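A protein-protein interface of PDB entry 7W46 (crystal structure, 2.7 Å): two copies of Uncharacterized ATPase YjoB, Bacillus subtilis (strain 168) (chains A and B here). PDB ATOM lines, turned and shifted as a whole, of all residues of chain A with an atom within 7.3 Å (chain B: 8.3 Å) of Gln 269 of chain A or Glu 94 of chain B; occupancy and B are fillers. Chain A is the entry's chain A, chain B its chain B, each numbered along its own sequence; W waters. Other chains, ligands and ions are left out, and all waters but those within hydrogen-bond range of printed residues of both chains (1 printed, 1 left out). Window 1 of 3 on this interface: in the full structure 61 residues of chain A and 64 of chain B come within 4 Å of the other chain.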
ATOM      1  N   ARG A 152      10.942   3.108 -13.761  1.00  0.00           N
ATOM      2  CA  ARG A 152      11.705   3.188 -15.000  1.00  0.00           C
ATOM      3  C   ARG A 152      13.135   2.719 -14.804  1.00  0.00           C
ATOM      4  O   ARG A 152      13.638   2.002 -15.683  1.00  0.00           O
ATOM      5  CB  ARG A 152      11.652   4.600 -15.606  1.00  0.00           C
ATOM      6  CG  ARG A 152      10.231   5.044 -16.008  1.00  0.00           C
ATOM      7  CD  ARG A 152       9.829   4.708 -17.459  1.00  0.00           C
ATOM      8  NE  ARG A 152       9.133   5.845 -18.086  1.00  0.00           N
ATOM      9  CZ  ARG A 152       7.918   5.796 -18.641  1.00  0.00           C
ATOM     10  NH1 ARG A 152       7.235   4.654 -18.666  1.00  0.00           N
ATOM     11  NH2 ARG A 152       7.379   6.896 -19.171  1.00  0.00           N
ATOM     12  N   PHE A 166      10.095  -3.905 -32.317  1.00  0.00           N
ATOM     13  CA  PHE A 166       8.815  -3.292 -32.641  1.00  0.00           C
ATOM     14  C   PHE A 166       8.535  -3.565 -34.102  1.00  0.00           C
ATOM     15  O   PHE A 166       9.351  -3.220 -34.965  1.00  0.00           O
ATOM     16  CB  PHE A 166       8.838  -1.785 -32.380  1.00  0.00           C
ATOM     17  CG  PHE A 166       9.120  -1.424 -30.959  1.00  0.00           C
ATOM     18  CD1 PHE A 166       8.101  -1.401 -30.026  1.00  0.00           C
ATOM     19  CD2 PHE A 166      10.408  -1.124 -30.549  1.00  0.00           C
ATOM     20  CE1 PHE A 166       8.361  -1.086 -28.715  1.00  0.00           C
ATOM     21  CE2 PHE A 166      10.675  -0.801 -29.231  1.00  0.00           C
ATOM     22  CZ  PHE A 166       9.651  -0.781 -28.315  1.00  0.00           C
ATOM     23  N   THR A 263       2.507   4.788 -36.196  1.00  0.00           N
ATOM     24  CA  THR A 263       3.449   3.802 -35.663  1.00  0.00           C
ATOM     25  C   THR A 263       4.791   4.448 -35.334  1.00  0.00           C
ATOM     26  O   THR A 263       5.446   4.047 -34.359  1.00  0.00           O
ATOM     27  CB  THR A 263       3.630   2.602 -36.624  1.00  0.00           C
ATOM     28  OG1 THR A 263       4.465   2.933 -37.747  1.00  0.00           O
ATOM     29  CG2 THR A 263       2.295   2.123 -37.151  1.00  0.00           C
ATOM     30  N   ILE A 264       5.197   5.470 -36.095  1.00  0.00           N
ATOM     31  CA  ILE A 264       6.422   6.192 -35.763  1.00  0.00           C
ATOM     32  C   ILE A 264       6.347   6.759 -34.353  1.00  0.00           C
ATOM     33  O   ILE A 264       7.208   6.477 -33.515  1.00  0.00           O
ATOM     34  CB  ILE A 264       6.710   7.288 -36.794  1.00  0.00           C
ATOM     35  CG1 ILE A 264       7.088   6.642 -38.135  1.00  0.00           C
ATOM     36  CG2 ILE A 264       7.836   8.148 -36.282  1.00  0.00           C
ATOM     37  CD1 ILE A 264       7.073   7.575 -39.337  1.00  0.00           C
ATOM     38  N   GLU A 265       5.299   7.533 -34.052  1.00  0.00           N
ATOM     39  CA  GLU A 265       5.206   8.145 -32.729  1.00  0.00           C
ATOM     40  C   GLU A 265       5.155   7.091 -31.634  1.00  0.00           C
ATOM     41  O   GLU A 265       5.778   7.245 -30.578  1.00  0.00           O
ATOM     42  CB  GLU A 265       3.994   9.086 -32.647  1.00  0.00           C
ATOM     43  CG  GLU A 265       4.341  10.489 -33.157  1.00  0.00           C
ATOM     44  CD  GLU A 265       3.763  11.638 -32.317  1.00  0.00           C
ATOM     45  OE1 GLU A 265       4.565  12.476 -31.819  1.00  0.00           O
ATOM     46  OE2 GLU A 265       2.510  11.723 -32.194  1.00  0.00           O
ATOM     47  N   GLU A 266       4.424   6.011 -31.868  1.00  0.00           N
ATOM     48  CA  GLU A 266       4.351   4.930 -30.892  1.00  0.00           C
ATOM     49  C   GLU A 266       5.737   4.353 -30.583  1.00  0.00           C
ATOM     50  O   GLU A 266       6.128   4.235 -29.410  1.00  0.00           O
ATOM     51  CB  GLU A 266       3.407   3.851 -31.420  1.00  0.00           C
ATOM     52  CG  GLU A 266       3.093   2.774 -30.420  1.00  0.00           C
ATOM     53  CD  GLU A 266       1.711   2.912 -29.835  1.00  0.00           C
ATOM     54  OE1 GLU A 266       0.771   3.096 -30.644  1.00  0.00           O
ATOM     55  OE2 GLU A 266       1.568   2.819 -28.587  1.00  0.00           O
ATOM     56  N   VAL A 267       6.507   4.010 -31.623  1.00  0.00           N
ATOM     57  CA  VAL A 267       7.803   3.362 -31.400  1.00  0.00           C
ATOM     58  C   VAL A 267       8.789   4.315 -30.719  1.00  0.00           C
ATOM     59  O   VAL A 267       9.509   3.927 -29.788  1.00  0.00           O
ATOM     60  CB  VAL A 267       8.371   2.819 -32.725  1.00  0.00           C
ATOM     61  CG1 VAL A 267       9.790   2.368 -32.529  1.00  0.00           C
ATOM     62  CG2 VAL A 267       7.526   1.687 -33.238  1.00  0.00           C
ATOM     63  N   PHE A 268       8.849   5.569 -31.171  1.00  0.00           N
ATOM     64  CA  PHE A 268       9.760   6.518 -30.542  1.00  0.00           C
ATOM     65  C   PHE A 268       9.400   6.761 -29.085  1.00  0.00           C
ATOM     66  O   PHE A 268      10.283   6.823 -28.221  1.00  0.00           O
ATOM     67  CB  PHE A 268       9.775   7.821 -31.327  1.00  0.00           C
ATOM     68  CG  PHE A 268      10.762   7.808 -32.432  1.00  0.00           C
ATOM     69  CD1 PHE A 268      10.473   7.177 -33.623  1.00  0.00           C
ATOM     70  CD2 PHE A 268      12.005   8.383 -32.268  1.00  0.00           C
ATOM     71  CE1 PHE A 268      11.404   7.149 -34.646  1.00  0.00           C
ATOM     72  CE2 PHE A 268      12.932   8.353 -33.280  1.00  0.00           C
ATOM     73  CZ  PHE A 268      12.631   7.734 -34.468  1.00  0.00           C
ATOM     74  N   GLN A 269       8.109   6.883 -28.784  1.00  0.00           N
ATOM     75  CA  GLN A 269       7.704   7.007 -27.391  1.00  0.00           C
ATOM     76  C   GLN A 269       8.133   5.792 -26.567  1.00  0.00           C
ATOM     77  O   GLN A 269       8.604   5.947 -25.433  1.00  0.00           O
ATOM     78  CB  GLN A 269       6.198   7.217 -27.309  1.00  0.00           C
ATOM     79  CG  GLN A 269       5.741   7.682 -25.946  1.00  0.00           C
ATOM     80  CD  GLN A 269       4.321   8.218 -25.957  1.00  0.00           C
ATOM     81  OE1 GLN A 269       3.817   8.697 -26.990  1.00  0.00           O
ATOM     82  NE2 GLN A 269       3.663   8.139 -24.801  1.00  0.00           N
ATOM     83  N   ALA A 270       7.993   4.576 -27.128  1.00  0.00           N
ATOM     84  CA  ALA A 270       8.357   3.363 -26.398  1.00  0.00           C
ATOM     85  C   ALA A 270       9.871   3.228 -26.236  1.00  0.00           C
ATOM     86  O   ALA A 270      10.355   2.865 -25.157  1.00  0.00           O
ATOM     87  CB  ALA A 270       7.787   2.127 -27.094  1.00  0.00           C
ATOM     88  N   ALA A 271      10.632   3.484 -27.299  1.00  0.00           N
ATOM     89  CA  ALA A 271      12.083   3.481 -27.169  1.00  0.00           C
ATOM     90  C   ALA A 271      12.533   4.510 -26.150  1.00  0.00           C
ATOM     91  O   ALA A 271      13.423   4.247 -25.330  1.00  0.00           O
ATOM     92  CB  ALA A 271      12.737   3.755 -28.520  1.00  0.00           C
ATOM     93  N   ARG A 272      11.914   5.689 -26.179  1.00  0.00           N
ATOM     94  CA  ARG A 272      12.296   6.763 -25.275  1.00  0.00           C
ATOM     95  C   ARG A 272      12.022   6.409 -23.829  1.00  0.00           C
ATOM     96  O   ARG A 272      12.679   6.953 -22.936  1.00  0.00           O
ATOM     97  CB  ARG A 272      11.553   8.039 -25.634  1.00  0.00           C
ATOM     98  CG  ARG A 272      12.392   9.258 -25.719  1.00  0.00           C
ATOM     99  CD  ARG A 272      11.628  10.298 -26.518  1.00  0.00           C
ATOM    100  NE  ARG A 272      12.139  10.514 -27.880  1.00  0.00           N
ATOM    101  CZ  ARG A 272      11.351  10.711 -28.941  1.00  0.00           C
ATOM    102  NH1 ARG A 272      10.005  10.696 -28.798  1.00  0.00           N
ATOM    103  NH2 ARG A 272      11.899  10.924 -30.140  1.00  0.00           N
ATOM    104  N   ARG A 273      11.065   5.517 -23.574  1.00  0.00           N
ATOM    105  CA  ARG A 273      10.837   5.080 -22.206  1.00  0.00           C
ATOM    106  C   ARG A 273      12.020   4.276 -21.673  1.00  0.00           C
ATOM    107  O   ARG A 273      12.178   4.148 -20.453  1.00  0.00           O
ATOM    108  CB  ARG A 273       9.534   4.284 -22.133  1.00  0.00           C
ATOM    109  CG  ARG A 273       8.299   5.166 -22.111  1.00  0.00           C
ATOM    110  CD  ARG A 273       7.014   4.420 -21.718  1.00  0.00           C
ATOM    111  NE  ARG A 273       6.577   3.451 -22.726  1.00  0.00           N
ATOM    112  CZ  ARG A 273       5.676   3.691 -23.676  1.00  0.00           C
ATOM    113  NH1 ARG A 273       5.090   4.883 -23.782  1.00  0.00           N
ATOM    114  NH2 ARG A 273       5.373   2.728 -24.534  1.00  0.00           N
ATOM    115  N   LEU A 274      12.865   3.760 -22.565  1.00  0.00           N
ATOM    116  CA  LEU A 274      14.054   3.008 -22.204  1.00  0.00           C
ATOM    117  C   LEU A 274      15.314   3.842 -22.316  1.00  0.00           C
ATOM    118  O   LEU A 274      16.405   3.271 -22.432  1.00  0.00           O
ATOM    119  CB  LEU A 274      14.187   1.765 -23.086  1.00  0.00           C
ATOM    120  CG  LEU A 274      12.957   0.858 -23.036  1.00  0.00           C
ATOM    121  CD1 LEU A 274      12.925  -0.076 -24.238  1.00  0.00           C
ATOM    122  CD2 LEU A 274      12.954   0.089 -21.725  1.00  0.00           C
ATOM    123  N   LEU A 308      17.960   9.056 -27.337  1.00  0.00           N
ATOM    124  CA  LEU A 308      18.106   7.930 -28.252  1.00  0.00           C
ATOM    125  C   LEU A 308      19.358   8.073 -29.100  1.00  0.00           C
ATOM    126  O   LEU A 308      19.665   9.158 -29.605  1.00  0.00           O
ATOM    127  CB  LEU A 308      16.891   7.792 -29.173  1.00  0.00           C
ATOM    128  CG  LEU A 308      15.551   7.420 -28.537  1.00  0.00           C
ATOM    129  CD1 LEU A 308      14.505   7.186 -29.605  1.00  0.00           C
ATOM    130  CD2 LEU A 308      15.660   6.229 -27.602  1.00  0.00           C
ATOM    131  N   ALA B  89      -0.421  11.253 -10.502  1.00  0.00           N
ATOM    132  CA  ALA B  89      -0.592  11.692 -11.880  1.00  0.00           C
ATOM    133  C   ALA B  89      -0.078  10.654 -12.870  1.00  0.00           C
ATOM    134  O   ALA B  89      -0.576  10.585 -13.996  1.00  0.00           O
ATOM    135  CB  ALA B  89       0.119  13.030 -12.072  1.00  0.00           C
ATOM    136  N   TYR B  90       0.874   9.816 -12.444  1.00  0.00           N
ATOM    137  CA  TYR B  90       1.685   8.949 -13.300  1.00  0.00           C
ATOM    138  C   TYR B  90       0.898   8.167 -14.334  1.00  0.00           C
ATOM    139  O   TYR B  90       0.169   7.228 -14.004  1.00  0.00           O
ATOM    140  CB  TYR B  90       2.486   7.972 -12.438  1.00  0.00           C
ATOM    141  CG  TYR B  90       3.363   6.989 -13.188  1.00  0.00           C
ATOM    142  CD1 TYR B  90       4.484   7.413 -13.893  1.00  0.00           C
ATOM    143  CD2 TYR B  90       3.088   5.628 -13.163  1.00  0.00           C
ATOM    144  CE1 TYR B  90       5.306   6.497 -14.562  1.00  0.00           C
ATOM    145  CE2 TYR B  90       3.891   4.710 -13.821  1.00  0.00           C
ATOM    146  CZ  TYR B  90       5.001   5.140 -14.516  1.00  0.00           C
ATOM    147  OH  TYR B  90       5.795   4.208 -15.165  1.00  0.00           O
ATOM    148  N   ASP B  91       1.058   8.548 -15.588  1.00  0.00           N
ATOM    149  CA  ASP B  91       0.455   7.854 -16.713  1.00  0.00           C
ATOM    150  C   ASP B  91       1.592   7.359 -17.600  1.00  0.00           C
ATOM    151  O   ASP B  91       2.335   8.162 -18.178  1.00  0.00           O
ATOM    152  CB  ASP B  91      -0.497   8.781 -17.468  1.00  0.00           C
ATOM    153  CG  ASP B  91      -1.568   8.028 -18.244  1.00  0.00           C
ATOM    154  OD1 ASP B  91      -1.404   6.801 -18.471  1.00  0.00           O
ATOM    155  OD2 ASP B  91      -2.568   8.676 -18.638  1.00  0.00           O
ATOM    156  N   GLU B  92       1.745   6.039 -17.687  1.00  0.00           N
ATOM    157  CA  GLU B  92       2.814   5.460 -18.491  1.00  0.00           C
ATOM    158  C   GLU B  92       2.629   5.703 -19.981  1.00  0.00           C
ATOM    159  O   GLU B  92       3.560   5.432 -20.747  1.00  0.00           O
ATOM    160  CB  GLU B  92       2.910   3.962 -18.219  1.00  0.00           C
ATOM    161  CG  GLU B  92       1.599   3.240 -18.405  1.00  0.00           C
ATOM    162  CD  GLU B  92       1.732   1.757 -18.194  1.00  0.00           C
ATOM    163  OE1 GLU B  92       2.457   1.367 -17.246  1.00  0.00           O
ATOM    164  OE2 GLU B  92       1.122   0.989 -18.976  1.00  0.00           O
ATOM    165  N   ASP B  93       1.455   6.201 -20.398  1.00  0.00           N
ATOM    166  CA  ASP B  93       1.190   6.533 -21.794  1.00  0.00           C
ATOM    167  C   ASP B  93       1.616   7.946 -22.175  1.00  0.00           C
ATOM    168  O   ASP B  93       1.825   8.199 -23.367  1.00  0.00           O
ATOM    169  CB  ASP B  93      -0.299   6.376 -22.121  1.00  0.00           C
ATOM    170  CG  ASP B  93      -0.826   4.982 -21.814  1.00  0.00           C
ATOM    171  OD1 ASP B  93      -0.071   3.992 -22.026  1.00  0.00           O
ATOM    172  OD2 ASP B  93      -1.999   4.892 -21.357  1.00  0.00           O
ATOM    173  N   GLU B  94       1.736   8.869 -21.208  1.00  0.00           N
ATOM    174  CA  GLU B  94       2.210  10.230 -21.477  1.00  0.00           C
ATOM    175  C   GLU B  94       3.730  10.277 -21.646  1.00  0.00           C
ATOM    176  O   GLU B  94       4.468   9.544 -20.978  1.00  0.00           O
ATOM    177  CB  GLU B  94       1.792  11.185 -20.356  1.00  0.00           C
ATOM    178  CG  GLU B  94       0.318  11.103 -19.977  1.00  0.00           C
ATOM    179  CD  GLU B  94      -0.483  12.305 -20.462  1.00  0.00           C
ATOM    180  OE1 GLU B  94       0.073  13.126 -21.228  1.00  0.00           O
ATOM    181  OE2 GLU B  94      -1.672  12.417 -20.084  1.00  0.00           O
ATOM    182  N   LYS B  95       4.191  11.156 -22.548  1.00  0.00           N
ATOM    183  CA  LYS B  95       5.624  11.259 -22.845  1.00  0.00           C
ATOM    184  C   LYS B  95       6.417  11.761 -21.643  1.00  0.00           C
ATOM    185  O   LYS B  95       7.509  11.249 -21.352  1.00  0.00           O
ATOM    186  CB  LYS B  95       5.859  12.179 -24.053  1.00  0.00           C
ATOM    187  CG  LYS B  95       5.108  11.794 -25.326  1.00  0.00           C
ATOM    188  CD  LYS B  95       5.300  12.818 -26.438  1.00  0.00           C
ATOM    189  CE  LYS B  95       4.605  12.391 -27.729  1.00  0.00           C
ATOM    190  NZ  LYS B  95       5.288  12.957 -28.938  1.00  0.00           N
ATOM    191  N   GLU B  96       5.897  12.786 -20.950  1.00  0.00           N
ATOM    192  CA  GLU B  96       6.475  13.252 -19.693  1.00  0.00           C
ATOM    193  C   GLU B  96       5.813  12.515 -18.527  1.00  0.00           C
ATOM    194  O   GLU B  96       4.573  12.481 -18.445  1.00  0.00           O
ATOM    195  CB  GLU B  96       6.319  14.769 -19.551  1.00  0.00           C
ATOM    196  CG  GLU B  96       5.092  15.374 -20.250  1.00  0.00           C
ATOM    197  CD  GLU B  96       5.204  16.904 -20.479  1.00  0.00           C
ATOM    198  OE1 GLU B  96       6.160  17.357 -21.180  1.00  0.00           O
ATOM    199  OE2 GLU B  96       4.341  17.651 -19.932  1.00  0.00           O
ATOM    200  N   PRO B  97       6.598  11.876 -17.643  1.00  0.00           N
ATOM    201  CA  PRO B  97       6.008  11.171 -16.498  1.00  0.00           C
ATOM    202  C   PRO B  97       5.876  12.079 -15.285  1.00  0.00           C
ATOM    203  O   PRO B  97       6.871  12.645 -14.823  1.00  0.00           O
ATOM    204  CB  PRO B  97       6.998  10.023 -16.238  1.00  0.00           C
ATOM    205  CG  PRO B  97       8.113  10.181 -17.285  1.00  0.00           C
ATOM    206  CD  PRO B  97       8.031  11.592 -17.773  1.00  0.00           C
ATOM    207  N   ASP B  98       4.658  12.231 -14.765  1.00  0.00           N
ATOM    208  CA  ASP B  98       4.380  13.060 -13.595  1.00  0.00           C
ATOM    209  C   ASP B  98       4.157  12.141 -12.399  1.00  0.00           C
ATOM    210  O   ASP B  98       3.197  11.367 -12.385  1.00  0.00           O
ATOM    211  CB  ASP B  98       3.155  13.948 -13.835  1.00  0.00           C
ATOM    212  CG  ASP B  98       3.024  15.084 -12.815  1.00  0.00           C
ATOM    213  OD1 ASP B  98       3.607  14.997 -11.720  1.00  0.00           O
ATOM    214  OD2 ASP B  98       2.319  16.076 -13.117  1.00  0.00           O
ATOM    215  N   LYS B 162       3.212  26.150 -21.314  1.00  0.00           N
ATOM    216  CA  LYS B 162       3.365  24.867 -21.966  1.00  0.00           C
ATOM    217  C   LYS B 162       3.368  25.121 -23.464  1.00  0.00           C
ATOM    218  O   LYS B 162       2.921  26.168 -23.934  1.00  0.00           O
ATOM    219  CB  LYS B 162       2.235  23.914 -21.567  1.00  0.00           C
ATOM    220  CG  LYS B 162       2.544  23.097 -20.311  1.00  0.00           C
ATOM    221  CD  LYS B 162       3.789  22.207 -20.508  1.00  0.00           C
ATOM    222  CE  LYS B 162       4.111  21.370 -19.269  1.00  0.00           C
ATOM    223  NZ  LYS B 162       3.069  20.340 -18.969  1.00  0.00           N
ATOM    224  N   ARG B 175      -4.025  16.407 -29.427  1.00  0.00           N
ATOM    225  CA  ARG B 175      -3.414  17.551 -28.766  1.00  0.00           C
ATOM    226  C   ARG B 175      -2.636  17.106 -27.528  1.00  0.00           C
ATOM    227  O   ARG B 175      -3.188  16.432 -26.657  1.00  0.00           O
ATOM    228  CB  ARG B 175      -4.482  18.576 -28.390  1.00  0.00           C
ATOM    229  CG  ARG B 175      -4.005  19.526 -27.336  1.00  0.00           C
ATOM    230  CD  ARG B 175      -4.914  20.741 -27.130  1.00  0.00           C
ATOM    231  NE  ARG B 175      -5.900  20.568 -26.065  1.00  0.00           N
ATOM    232  CZ  ARG B 175      -5.615  20.256 -24.801  1.00  0.00           C
ATOM    233  NH1 ARG B 175      -4.357  20.059 -24.408  1.00  0.00           N
ATOM    234  NH2 ARG B 175      -6.602  20.122 -23.919  1.00  0.00           N
ATOM    235  N   GLU B 176      -1.351  17.468 -27.460  1.00  0.00           N
ATOM    236  CA  GLU B 176      -0.535  17.262 -26.265  1.00  0.00           C
ATOM    237  C   GLU B 176       0.135  18.567 -25.864  1.00  0.00           C
ATOM    238  O   GLU B 176       0.556  19.346 -26.723  1.00  0.00           O
ATOM    239  CB  GLU B 176       0.541  16.189 -26.473  1.00  0.00           C
ATOM    240  CG  GLU B 176       0.017  14.756 -26.361  1.00  0.00           C
ATOM    241  CD  GLU B 176       1.143  13.726 -26.203  1.00  0.00           C
ATOM    242  OE1 GLU B 176       1.519  13.409 -25.047  1.00  0.00           O
ATOM    243  OE2 GLU B 176       1.649  13.227 -27.240  1.00  0.00           O
ATOM    244  N   GLN B 177       0.238  18.803 -24.557  1.00  0.00           N
ATOM    245  CA  GLN B 177       0.945  19.956 -24.016  1.00  0.00           C
ATOM    246  C   GLN B 177       2.266  19.480 -23.441  1.00  0.00           C
ATOM    247  O   GLN B 177       2.288  18.615 -22.561  1.00  0.00           O
ATOM    248  CB  GLN B 177       0.104  20.669 -22.965  1.00  0.00           C
ATOM    249  CG  GLN B 177      -1.155  21.272 -23.578  1.00  0.00           C
ATOM    250  CD  GLN B 177      -1.842  22.298 -22.683  1.00  0.00           C
ATOM    251  OE1 GLN B 177      -3.045  22.551 -22.830  1.00  0.00           O
ATOM    252  NE2 GLN B 177      -1.082  22.899 -21.753  1.00  0.00           N
ATOM    253  N   GLU B 178       3.360  20.020 -23.962  1.00  0.00           N
ATOM    254  CA  GLU B 178       4.714  19.658 -23.580  1.00  0.00           C
ATOM    255  C   GLU B 178       5.461  20.888 -23.095  1.00  0.00           C
ATOM    256  O   GLU B 178       5.017  22.027 -23.257  1.00  0.00           O
ATOM    257  CB  GLU B 178       5.492  19.052 -24.759  1.00  0.00           C
ATOM    258  CG  GLU B 178       4.645  18.392 -25.838  1.00  0.00           C
ATOM    259  CD  GLU B 178       5.471  17.565 -26.835  1.00  0.00           C
ATOM    260  OE1 GLU B 178       6.605  17.989 -27.193  1.00  0.00           O
ATOM    261  OE2 GLU B 178       4.985  16.481 -27.251  1.00  0.00           O
HETATM  262  O   HOH W   1       6.730  10.225 -30.375  1.00  0.00           O
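The backbone carbonyl oxygen of Asp 98 of chain B sits at hydrogen-bond distance from the backbone NH of Tyr 90 of chain B, at 2.8 Å. N of Asp 93 of chain B sits close to OD1 of Asp 91 of chain B, at 3.5 Å. The side-chain amino group (NZ) of Lys 95 of chain B lies within salt-bridge range of the side-chain carboxylate (OE2) of Glu 178 of chain B (3.9 Å).
Printed residues of chain B within 4 Å of Arg 152 of chain A: Tyr 90 and Pro 97. Printed residues of chain B within 4 Å of Glu 265 of chain A: Lys 95. Val 267 of chain A touches none of the printed residues of chain B. Gln 269 of chain A touches just these residues of chain B: Asp 93 (2.3 Å), Glu 94 (3.8 Å) and Lys 95 (3.7 Å). Leu 274 of chain A touches none of the printed residues of chain B. Of the printed residues of chain A, Asp 93 of chain B touches Gln 269. Printed residues of chain A within 4 Å of Glu 94 of chain B: Gln 269 (3.8 Å). The nearest residue of chain A that does not touch Glu 94 of chain B is Arg 152 of chain A (4.3 Å). The nearest printed residue of chain B that does not touch Arg 152 of chain A is Glu 92 of chain B (4.3 Å).
Printed residues of chain B that touch a printed residue of chain A: Tyr 90, Glu 92, Asp 93, Glu 94, Lys 95 and Pro 97. Of the 15 printed residues of chain A, 4 touch a printed residue of chain B. Among the printed residues, 7 pairs touch across the chains. Among the printed residues, Asp or Glu carboxylates within 4 Å of a Lys or Arg side-chain nitrogen of the other chain: Glu 265 of chain A with Lys 95 of chain B (3.0 Å).
No position is printed for both chains. Of the 7 pairs that touch across the chains among the printed residues, none has its exchanged pair printed and touching as well.
Tyr 90 of chain B touches Arg 152 of chain A. NH2 of Arg 152 of chain A touches CG of Pro 97 of chain B, at 3.9 Å. C of Glu 94 of chain B touches NE2 of Gln 269 of chain A, 3.8 Å away. Gln 269 of chain A touches Lys 95 of chain B (CD to CG, 3.7 Å).
The side-chain carboxylate (OE1) of Glu 265 of chain A lies within salt-bridge range of the side-chain amino group (NZ) of Lys 95 of chain B, 3.0 Å away. The backbone carbonyl oxygen of Glu 92 of chain B lies within hydrogen-bond range of the guanidinium group of Arg 273 of chain A (3.4 Å). The backbone carbonyl oxygen (O) of Asp 93 of chain B sits close to the side-chain amide nitrogen (NE2) of Gln 269 of chain A, at 2.3 Å.
Water W1 bridges the backbone carbonyl oxygen (O) of Glu 265 of chain A and the side-chain amino group (NZ) of Lys 95 of chain B.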
